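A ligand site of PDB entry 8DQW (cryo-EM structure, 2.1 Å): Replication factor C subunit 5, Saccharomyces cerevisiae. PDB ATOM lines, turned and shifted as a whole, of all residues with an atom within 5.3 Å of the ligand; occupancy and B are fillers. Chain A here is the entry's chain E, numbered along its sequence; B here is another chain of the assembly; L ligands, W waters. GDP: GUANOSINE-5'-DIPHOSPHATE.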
ATOM      1  N   VAL A   5      24.427  21.216 -12.105  1.00  0.00           N
ATOM      2  CA  VAL A   5      24.408  22.672 -12.244  1.00  0.00           C
ATOM      3  C   VAL A   5      24.051  23.071 -13.668  1.00  0.00           C
ATOM      4  O   VAL A   5      23.319  24.039 -13.900  1.00  0.00           O
ATOM      5  CB  VAL A   5      25.763  23.277 -11.821  1.00  0.00           C
ATOM      6  CG1 VAL A   5      26.027  23.020 -10.338  1.00  0.00           C
ATOM      7  CG2 VAL A   5      26.898  22.724 -12.669  1.00  0.00           C
ATOM      8  N   ASP A   6      24.562  22.314 -14.653  1.00  0.00           N
ATOM      9  CA  ASP A   6      24.282  22.573 -16.051  1.00  0.00           C
ATOM     10  C   ASP A   6      23.144  21.720 -16.614  1.00  0.00           C
ATOM     11  O   ASP A   6      22.501  22.131 -17.578  1.00  0.00           O
ATOM     12  CB  ASP A   6      25.535  22.339 -16.902  1.00  0.00           C
ATOM     13  CG  ASP A   6      26.755  23.066 -16.358  1.00  0.00           C
ATOM     14  OD1 ASP A   6      26.606  24.240 -15.933  1.00  0.00           O
ATOM     15  OD2 ASP A   6      27.854  22.471 -16.343  1.00  0.00           O
ATOM     16  N   TYR A   8      20.127  20.845 -15.462  1.00  0.00           N
ATOM     17  CA  TYR A   8      18.783  21.401 -15.294  1.00  0.00           C
ATOM     18  C   TYR A   8      18.783  22.921 -15.404  1.00  0.00           C
ATOM     19  O   TYR A   8      17.908  23.579 -14.842  1.00  0.00           O
ATOM     20  CB  TYR A   8      18.188  20.966 -13.961  1.00  0.00           C
ATOM     21  CG  TYR A   8      18.120  19.458 -13.779  1.00  0.00           C
ATOM     22  CD1 TYR A   8      19.223  18.756 -13.300  1.00  0.00           C
ATOM     23  CD2 TYR A   8      16.974  18.752 -14.083  1.00  0.00           C
ATOM     24  CE1 TYR A   8      19.171  17.387 -13.129  1.00  0.00           C
ATOM     25  CE2 TYR A   8      16.910  17.383 -13.920  1.00  0.00           C
ATOM     26  CZ  TYR A   8      18.005  16.712 -13.434  1.00  0.00           C
ATOM     27  OH  TYR A   8      17.951  15.342 -13.272  1.00  0.00           O
ATOM     28  N   ARG A   9      19.744  23.481 -16.123  1.00  0.00           N
ATOM     29  CA  ARG A   9      19.804  24.923 -16.274  1.00  0.00           C
ATOM     30  C   ARG A   9      18.658  25.398 -17.166  1.00  0.00           C
ATOM     31  O   ARG A   9      18.479  24.866 -18.273  1.00  0.00           O
ATOM     32  CB  ARG A   9      21.156  25.337 -16.870  1.00  0.00           C
ATOM     33  CG  ARG A   9      21.167  26.695 -17.565  1.00  0.00           C
ATOM     34  CD  ARG A   9      22.455  27.445 -17.282  1.00  0.00           C
ATOM     35  NE  ARG A   9      22.754  28.424 -18.317  1.00  0.00           N
ATOM     36  CZ  ARG A   9      23.979  28.819 -18.641  1.00  0.00           C
ATOM     37  NH1 ARG A   9      25.049  28.360 -18.015  1.00  0.00           N
ATOM     38  NH2 ARG A   9      24.121  29.710 -19.616  1.00  0.00           N
ATOM     39  N   PRO A  10      17.860  26.369 -16.731  1.00  0.00           N
ATOM     40  CA  PRO A  10      16.781  26.866 -17.597  1.00  0.00           C
ATOM     41  C   PRO A  10      17.327  27.428 -18.898  1.00  0.00           C
ATOM     42  O   PRO A  10      18.408  28.018 -18.935  1.00  0.00           O
ATOM     43  CB  PRO A  10      16.089  27.952 -16.756  1.00  0.00           C
ATOM     44  CG  PRO A  10      16.542  27.717 -15.362  1.00  0.00           C
ATOM     45  CD  PRO A  10      17.887  27.073 -15.436  1.00  0.00           C
ATOM     46  N   ALA A  15      11.240  29.645 -18.219  1.00  0.00           N
ATOM     47  CA  ALA A  15      11.728  28.568 -17.364  1.00  0.00           C
ATOM     48  C   ALA A  15      12.345  29.073 -16.067  1.00  0.00           C
ATOM     49  O   ALA A  15      12.627  28.257 -15.189  1.00  0.00           O
ATOM     50  CB  ALA A  15      12.751  27.727 -18.123  1.00  0.00           C
ATOM     51  N   LEU A  16      12.559  30.378 -15.931  1.00  0.00           N
ATOM     52  CA  LEU A  16      13.078  30.920 -14.682  1.00  0.00           C
ATOM     53  C   LEU A  16      12.060  30.709 -13.569  1.00  0.00           C
ATOM     54  O   LEU A  16      10.859  30.899 -13.757  1.00  0.00           O
ATOM     55  CB  LEU A  16      13.404  32.404 -14.836  1.00  0.00           C
ATOM     56  CG  LEU A  16      14.362  32.754 -15.977  1.00  0.00           C
ATOM     57  CD1 LEU A  16      14.392  34.257 -16.203  1.00  0.00           C
ATOM     58  CD2 LEU A  16      15.755  32.218 -15.696  1.00  0.00           C
ATOM     59  N   SER A  17      12.550  30.323 -12.386  1.00  0.00           N
ATOM     60  CA  SER A  17      11.683  29.924 -11.285  1.00  0.00           C
ATOM     61  C   SER A  17      11.843  30.769 -10.033  1.00  0.00           C
ATOM     62  O   SER A  17      11.115  30.541  -9.062  1.00  0.00           O
ATOM     63  CB  SER A  17      11.922  28.452 -10.927  1.00  0.00           C
ATOM     64  OG  SER A  17      13.293  28.205 -10.680  1.00  0.00           O
ATOM     65  N   HIS A  18      12.761  31.736 -10.009  1.00  0.00           N
ATOM     66  CA  HIS A  18      12.924  32.617  -8.865  1.00  0.00           C
ATOM     67  C   HIS A  18      13.119  34.049  -9.346  1.00  0.00           C
ATOM     68  O   HIS A  18      13.557  34.295 -10.473  1.00  0.00           O
ATOM     69  CB  HIS A  18      14.112  32.181  -7.975  1.00  0.00           C
ATOM     70  CG  HIS A  18      15.455  32.519  -8.539  1.00  0.00           C
ATOM     71  ND1 HIS A  18      16.055  33.746  -8.380  1.00  0.00           N
ATOM     72  CD2 HIS A  18      16.342  31.761  -9.233  1.00  0.00           C
ATOM     73  CE1 HIS A  18      17.235  33.743  -8.961  1.00  0.00           C
ATOM     74  NE2 HIS A  18      17.438  32.554  -9.485  1.00  0.00           N
ATOM     75  N   PRO A  44      24.954  39.039  -6.311  1.00  0.00           N
ATOM     76  CA  PRO A  44      25.812  38.030  -5.686  1.00  0.00           C
ATOM     77  C   PRO A  44      26.164  36.906  -6.656  1.00  0.00           C
ATOM     78  O   PRO A  44      25.392  36.553  -7.546  1.00  0.00           O
ATOM     79  CB  PRO A  44      24.970  37.508  -4.522  1.00  0.00           C
ATOM     80  CG  PRO A  44      23.902  38.509  -4.299  1.00  0.00           C
ATOM     81  CD  PRO A  44      23.715  39.289  -5.558  1.00  0.00           C
ATOM     82  N   ASN A  45      27.355  36.351  -6.479  1.00  0.00           N
ATOM     83  CA  ASN A  45      27.840  35.298  -7.348  1.00  0.00           C
ATOM     84  C   ASN A  45      26.984  34.039  -7.211  1.00  0.00           C
ATOM     85  O   ASN A  45      26.474  33.728  -6.135  1.00  0.00           O
ATOM     86  CB  ASN A  45      29.299  34.967  -7.034  1.00  0.00           C
ATOM     87  CG  ASN A  45      29.911  33.995  -8.020  1.00  0.00           C
ATOM     88  OD1 ASN A  45      29.575  34.013  -9.201  1.00  0.00           O
ATOM     89  ND2 ASN A  45      30.804  33.148  -7.535  1.00  0.00           N
ATOM     90  N   GLY A  46      26.815  33.334  -8.327  1.00  0.00           N
ATOM     91  CA  GLY A  46      26.081  32.084  -8.315  1.00  0.00           C
ATOM     92  C   GLY A  46      24.578  32.227  -8.176  1.00  0.00           C
ATOM     93  O   GLY A  46      23.923  31.287  -7.738  1.00  0.00           O
ATOM     94  N   THR A  47      24.017  33.385  -8.537  1.00  0.00           N
ATOM     95  CA  THR A  47      22.584  33.602  -8.430  1.00  0.00           C
ATOM     96  C   THR A  47      21.827  33.334  -9.724  1.00  0.00           C
ATOM     97  O   THR A  47      20.615  33.084  -9.667  1.00  0.00           O
ATOM     98  CB  THR A  47      22.301  35.047  -7.977  1.00  0.00           C
ATOM     99  OG1 THR A  47      22.958  35.966  -8.863  1.00  0.00           O
ATOM    100  CG2 THR A  47      22.792  35.269  -6.558  1.00  0.00           C
ATOM    101  N   GLY A  48      22.506  33.369 -10.865  1.00  0.00           N
ATOM    102  CA  GLY A  48      21.864  33.101 -12.138  1.00  0.00           C
ATOM    103  C   GLY A  48      21.919  34.257 -13.112  1.00  0.00           C
ATOM    104  O   GLY A  48      21.051  34.372 -13.995  1.00  0.00           O
ATOM    105  N   LYS A  49      22.923  35.126 -12.978  1.00  0.00           N
ATOM    106  CA  LYS A  49      23.040  36.270 -13.879  1.00  0.00           C
ATOM    107  C   LYS A  49      23.328  35.813 -15.304  1.00  0.00           C
ATOM    108  O   LYS A  49      22.668  36.255 -16.259  1.00  0.00           O
ATOM    109  CB  LYS A  49      24.141  37.216 -13.383  1.00  0.00           C
ATOM    110  CG  LYS A  49      23.903  37.759 -11.988  1.00  0.00           C
ATOM    111  CD  LYS A  49      24.949  38.802 -11.608  1.00  0.00           C
ATOM    112  CE  LYS A  49      26.311  38.199 -11.302  1.00  0.00           C
ATOM    113  NZ  LYS A  49      26.252  37.012 -10.406  1.00  0.00           N
ATOM    114  N   LYS A  50      24.319  34.932 -15.478  1.00  0.00           N
ATOM    115  CA  LYS A  50      24.631  34.426 -16.810  1.00  0.00           C
ATOM    116  C   LYS A  50      23.461  33.670 -17.410  1.00  0.00           C
ATOM    117  O   LYS A  50      23.177  33.774 -18.613  1.00  0.00           O
ATOM    118  CB  LYS A  50      25.875  33.540 -16.752  1.00  0.00           C
ATOM    119  CG  LYS A  50      26.399  33.085 -18.108  1.00  0.00           C
ATOM    120  CD  LYS A  50      26.882  34.247 -18.954  1.00  0.00           C
ATOM    121  CE  LYS A  50      27.619  33.772 -20.192  1.00  0.00           C
ATOM    122  NZ  LYS A  50      28.888  33.064 -19.865  1.00  0.00           N
ATOM    123  N   THR A  51      22.760  32.885 -16.585  1.00  0.00           N
ATOM    124  CA  THR A  51      21.574  32.177 -17.056  1.00  0.00           C
ATOM    125  C   THR A  51      20.522  33.157 -17.561  1.00  0.00           C
ATOM    126  O   THR A  51      19.912  32.929 -18.609  1.00  0.00           O
ATOM    127  CB  THR A  51      21.001  31.318 -15.937  1.00  0.00           C
ATOM    128  OG1 THR A  51      21.960  30.313 -15.556  1.00  0.00           O
ATOM    129  CG2 THR A  51      19.711  30.638 -16.372  1.00  0.00           C
ATOM    130  N   ARG A  52      20.308  34.253 -16.838  1.00  0.00           N
ATOM    131  CA  ARG A  52      19.321  35.242 -17.263  1.00  0.00           C
ATOM    132  C   ARG A  52      19.755  35.941 -18.551  1.00  0.00           C
ATOM    133  O   ARG A  52      18.927  36.218 -19.423  1.00  0.00           O
ATOM    134  CB  ARG A  52      19.080  36.252 -16.145  1.00  0.00           C
ATOM    135  CG  ARG A  52      17.860  35.931 -15.288  1.00  0.00           C
ATOM    136  CD  ARG A  52      18.119  36.188 -13.811  1.00  0.00           C
ATOM    137  NE  ARG A  52      17.134  35.526 -12.961  1.00  0.00           N
ATOM    138  CZ  ARG A  52      17.119  34.227 -12.714  1.00  0.00           C
ATOM    139  NH1 ARG A  52      18.035  33.414 -13.222  1.00  0.00           N
ATOM    140  NH2 ARG A  52      16.157  33.724 -11.951  1.00  0.00           N
ATOM    141  N   VAL A 170      28.595  41.523 -16.962  1.00  0.00           N
ATOM    142  CA  VAL A 170      28.140  40.846 -15.744  1.00  0.00           C
ATOM    143  C   VAL A 170      29.217  41.002 -14.678  1.00  0.00           C
ATOM    144  O   VAL A 170      30.408  40.799 -14.958  1.00  0.00           O
ATOM    145  CB  VAL A 170      27.854  39.353 -16.007  1.00  0.00           C
ATOM    146  CG1 VAL A 170      27.144  38.740 -14.813  1.00  0.00           C
ATOM    147  CG2 VAL A 170      27.037  39.182 -17.271  1.00  0.00           C
ATOM    148  N   ILE A 201      14.027  24.318  -5.910  1.00  0.00           N
ATOM    149  CA  ILE A 201      14.834  23.876  -7.042  1.00  0.00           C
ATOM    150  C   ILE A 201      15.523  22.559  -6.714  1.00  0.00           C
ATOM    151  O   ILE A 201      15.545  21.617  -7.535  1.00  0.00           O
ATOM    152  CB  ILE A 201      15.839  24.964  -7.439  1.00  0.00           C
ATOM    153  CG1 ILE A 201      15.110  26.204  -7.975  1.00  0.00           C
ATOM    154  CG2 ILE A 201      16.820  24.429  -8.477  1.00  0.00           C
ATOM    155  CD1 ILE A 201      15.976  27.434  -8.100  1.00  0.00           C
ATOM    156  N   LEU A 230      23.352  29.332  -5.633  1.00  0.00           N
ATOM    157  CA  LEU A 230      22.614  28.191  -6.148  1.00  0.00           C
ATOM    158  C   LEU A 230      23.539  27.159  -6.772  1.00  0.00           C
ATOM    159  O   LEU A 230      23.328  25.944  -6.623  1.00  0.00           O
ATOM    160  CB  LEU A 230      21.587  28.674  -7.175  1.00  0.00           C
ATOM    161  CG  LEU A 230      20.541  27.683  -7.695  1.00  0.00           C
ATOM    162  CD1 LEU A 230      19.958  26.824  -6.574  1.00  0.00           C
ATOM    163  CD2 LEU A 230      19.437  28.422  -8.424  1.00  0.00           C
ATOM    164  N   ARG A 231      24.578  27.617  -7.481  1.00  0.00           N
ATOM    165  CA  ARG A 231      25.535  26.690  -8.073  1.00  0.00           C
ATOM    166  C   ARG A 231      26.191  25.818  -7.010  1.00  0.00           C
ATOM    167  O   ARG A 231      26.295  24.594  -7.152  1.00  0.00           O
ATOM    168  CB  ARG A 231      26.588  27.470  -8.859  1.00  0.00           C
ATOM    169  CG  ARG A 231      27.772  26.653  -9.342  1.00  0.00           C
ATOM    170  CD  ARG A 231      28.671  27.459 -10.267  1.00  0.00           C
ATOM    171  NE  ARG A 231      29.094  28.721  -9.671  1.00  0.00           N
ATOM    172  CZ  ARG A 231      28.650  29.918 -10.017  1.00  0.00           C
ATOM    173  NH1 ARG A 231      27.749  30.082 -10.983  1.00  0.00           N
ATOM    174  NH2 ARG A 231      29.111  30.992  -9.382  1.00  0.00           N
ATOM    175  N   LEU A 234      23.695  23.217  -5.671  1.00  0.00           N
ATOM    176  CA  LEU A 234      23.545  22.042  -6.533  1.00  0.00           C
ATOM    177  C   LEU A 234      24.789  21.156  -6.475  1.00  0.00           C
ATOM    178  O   LEU A 234      24.665  19.919  -6.462  1.00  0.00           O
ATOM    179  CB  LEU A 234      23.269  22.487  -7.967  1.00  0.00           C
ATOM    180  CG  LEU A 234      21.881  23.103  -8.188  1.00  0.00           C
ATOM    181  CD1 LEU A 234      21.859  23.995  -9.409  1.00  0.00           C
ATOM    182  CD2 LEU A 234      20.828  22.006  -8.303  1.00  0.00           C
ATOM    183  N   ASN B 479      35.315  30.621 -11.004  1.00  0.00           N
ATOM    184  CA  ASN B 479      34.458  29.596 -10.416  1.00  0.00           C
ATOM    185  C   ASN B 479      35.195  28.270 -10.280  1.00  0.00           C
ATOM    186  O   ASN B 479      34.896  27.496  -9.365  1.00  0.00           O
ATOM    187  CB  ASN B 479      33.203  29.412 -11.272  1.00  0.00           C
ATOM    188  CG  ASN B 479      32.217  30.556 -11.093  1.00  0.00           C
ATOM    189  OD1 ASN B 479      32.225  31.251 -10.080  1.00  0.00           O
ATOM    190  ND2 ASN B 479      31.345  30.747 -12.078  1.00  0.00           N
HETATM  191  PB  GDP L   1      25.842  33.681 -11.938  1.00  0.00           P
HETATM  192  O1B GDP L   1      25.340  34.745 -10.995  1.00  0.00           O
HETATM  193  O2B GDP L   1      27.186  33.171 -11.477  1.00  0.00           O
HETATM  194  O3B GDP L   1      25.977  34.253 -13.330  1.00  0.00           O
HETATM  195  O3A GDP L   1      24.748  32.448 -11.956  1.00  0.00           O
HETATM  196  PA  GDP L   1      24.967  30.993 -12.714  1.00  0.00           P
HETATM  197  O1A GDP L   1      24.018  30.899 -13.883  1.00  0.00           O
HETATM  198  O2A GDP L   1      26.389  30.874 -13.211  1.00  0.00           O
HETATM  199  O5' GDP L   1      24.655  29.799 -11.628  1.00  0.00           O
HETATM  200  C5' GDP L   1      23.318  29.550 -11.293  1.00  0.00           C
HETATM  201  C4' GDP L   1      23.035  28.064 -11.362  1.00  0.00           C
HETATM  202  O4' GDP L   1      21.541  27.779 -10.809  1.00  0.00           O
HETATM  203  C3' GDP L   1      23.085  27.631 -12.584  1.00  0.00           C
HETATM  204  O3' GDP L   1      23.656  26.246 -12.625  1.00  0.00           O
HETATM  205  C2' GDP L   1      21.624  27.612 -13.097  1.00  0.00           C
HETATM  206  O2' GDP L   1      21.406  26.496 -13.841  1.00  0.00           O
HETATM  207  C1' GDP L   1      20.744  27.581 -11.827  1.00  0.00           C
HETATM  208  N9  GDP L   1      19.723  28.642 -11.887  1.00  0.00           N
HETATM  209  C8  GDP L   1      19.870  29.970 -11.967  1.00  0.00           C
HETATM  210  N7  GDP L   1      18.634  30.507 -11.990  1.00  0.00           N
HETATM  211  C5  GDP L   1      17.750  29.511 -11.924  1.00  0.00           C
HETATM  212  C6  GDP L   1      16.216  29.496 -11.912  1.00  0.00           C
HETATM  213  O6  GDP L   1      15.610  30.515 -11.969  1.00  0.00           O
HETATM  214  N1  GDP L   1      15.514  28.254 -11.835  1.00  0.00           N
HETATM  215  C2  GDP L   1      16.253  27.020 -11.773  1.00  0.00           C
HETATM  216  N2  GDP L   1      15.550  25.748 -11.693  1.00  0.00           N
HETATM  217  N3  GDP L   1      17.715  27.037 -11.783  1.00  0.00           N
HETATM  218  C4  GDP L   1      18.441  28.329 -11.860  1.00  0.00           C
HETATM  219  O   HOH W   1      28.183  31.695 -14.719  1.00  0.00           O
HETATM  220  O   HOH W   2      30.015  33.575 -11.989  1.00  0.00           O
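The side-chain amino group (NZ) of Lys 49 sits at hydrogen-bond distance from the backbone carbonyl oxygen (O) of Pro 44 (3.0 Å). The guanidinium group of Arg 9 sits close to the side-chain hydroxyl of Thr 51 (3.4 Å). NH2 of Arg 231 sits at hydrogen-bond distance from OD1 of Asn 45, at 3.1 Å. NH2 of Arg 231 sits at hydrogen-bond distance from OD1 of Asn 479 of chain B (3.2 Å). A ring nitrogen (NE2) of His 18 lies within hydrogen-bond range of the guanidinium group of Arg 52, 3.0 Å away. The side-chain hydroxyl of Thr 47 sits at hydrogen-bond distance from the backbone carbonyl oxygen of Pro 44 (2.8 Å). The backbone carbonyl oxygen (O) of Gly 46 sits at hydrogen-bond distance from the backbone NH (N) of Leu 230. OD1 of Asn 479 of chain B lies within hydrogen-bond range of ND2 of Asn 45, 3.5 Å away.
CB of Arg 9 touches O2' of the ligand, 3.3 Å away. CD of Pro 10 touches N3 of the ligand (3.7 Å). Leu 16 touches the ligand. Pro 44 touches the ligand (O to O1B, 3.9 Å). Ile 201 touches the ligand (CG2 to N2, 3.7 Å). CD2 of Leu 230 touches O4' of the ligand (3.2 Å). Hydrophobic or aromatic side chains that line the ligand: Val 5, Pro 10, His 18, Ile 201 and Leu 230. Of the 24 residues printed, 18 come within 4 Å of the ligand.
An oxygen (O6) of the ligand sits at hydrogen-bond distance from the backbone NH (N) of Ser 17 (3.1 Å). OG of Ser 17 sits at hydrogen-bond distance from N1 of the ligand, 2.5 Å away. N of Lys 49 is in hydrogen-bond range of O1B of the ligand. The side-chain amino group (NZ) of Lys 49 lies within salt-bridge range of an oxygen (O1B) of the ligand. The backbone carbonyl oxygen (O) of Val 5 sits at hydrogen-bond distance from an oxygen (O3') of the ligand (2.6 Å). The backbone NH (N) of Gly 48 is in hydrogen-bond range of an oxygen (O3A) of the ligand (2.7 Å). The side-chain hydroxyl of Thr 51 is in hydrogen-bond range of an oxygen (O1A) of the ligand. O2A of the ligand is in salt-bridge range of NH1 of Arg 231, at 2.7 Å. The backbone NH (N) of Lys 50 sits at hydrogen-bond distance from an oxygen (O3B) of the ligand (2.8 Å). NE2 of His 18 is in hydrogen-bond range of N7 of the ligand (3.4 Å). The backbone NH of Thr 47 lies within hydrogen-bond range of an oxygen (O1B) of the ligand, at 3.1 Å. The side-chain hydroxyl (OG1) of Thr 47 lies within hydrogen-bond range of an oxygen (O1B) of the ligand. N of Gly 46 lies within hydrogen-bond range of O2B of the ligand, at 3.2 Å. NH1 of Arg 52 lies within hydrogen-bond range of N7 of the ligand. An oxygen (O2B) of the ligand lies close to the side-chain amide oxygen (OD1) of Asn 45, 3.4 Å away.
Water W2 lies within hydrogen-bond range of the side-chain amide oxygen of Asn 45 (2.9 Å), an oxygen (O2B) of the ligand (2.9 Å) and the side-chain amide nitrogen of Asn 479 of chain B (3.1 Å).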
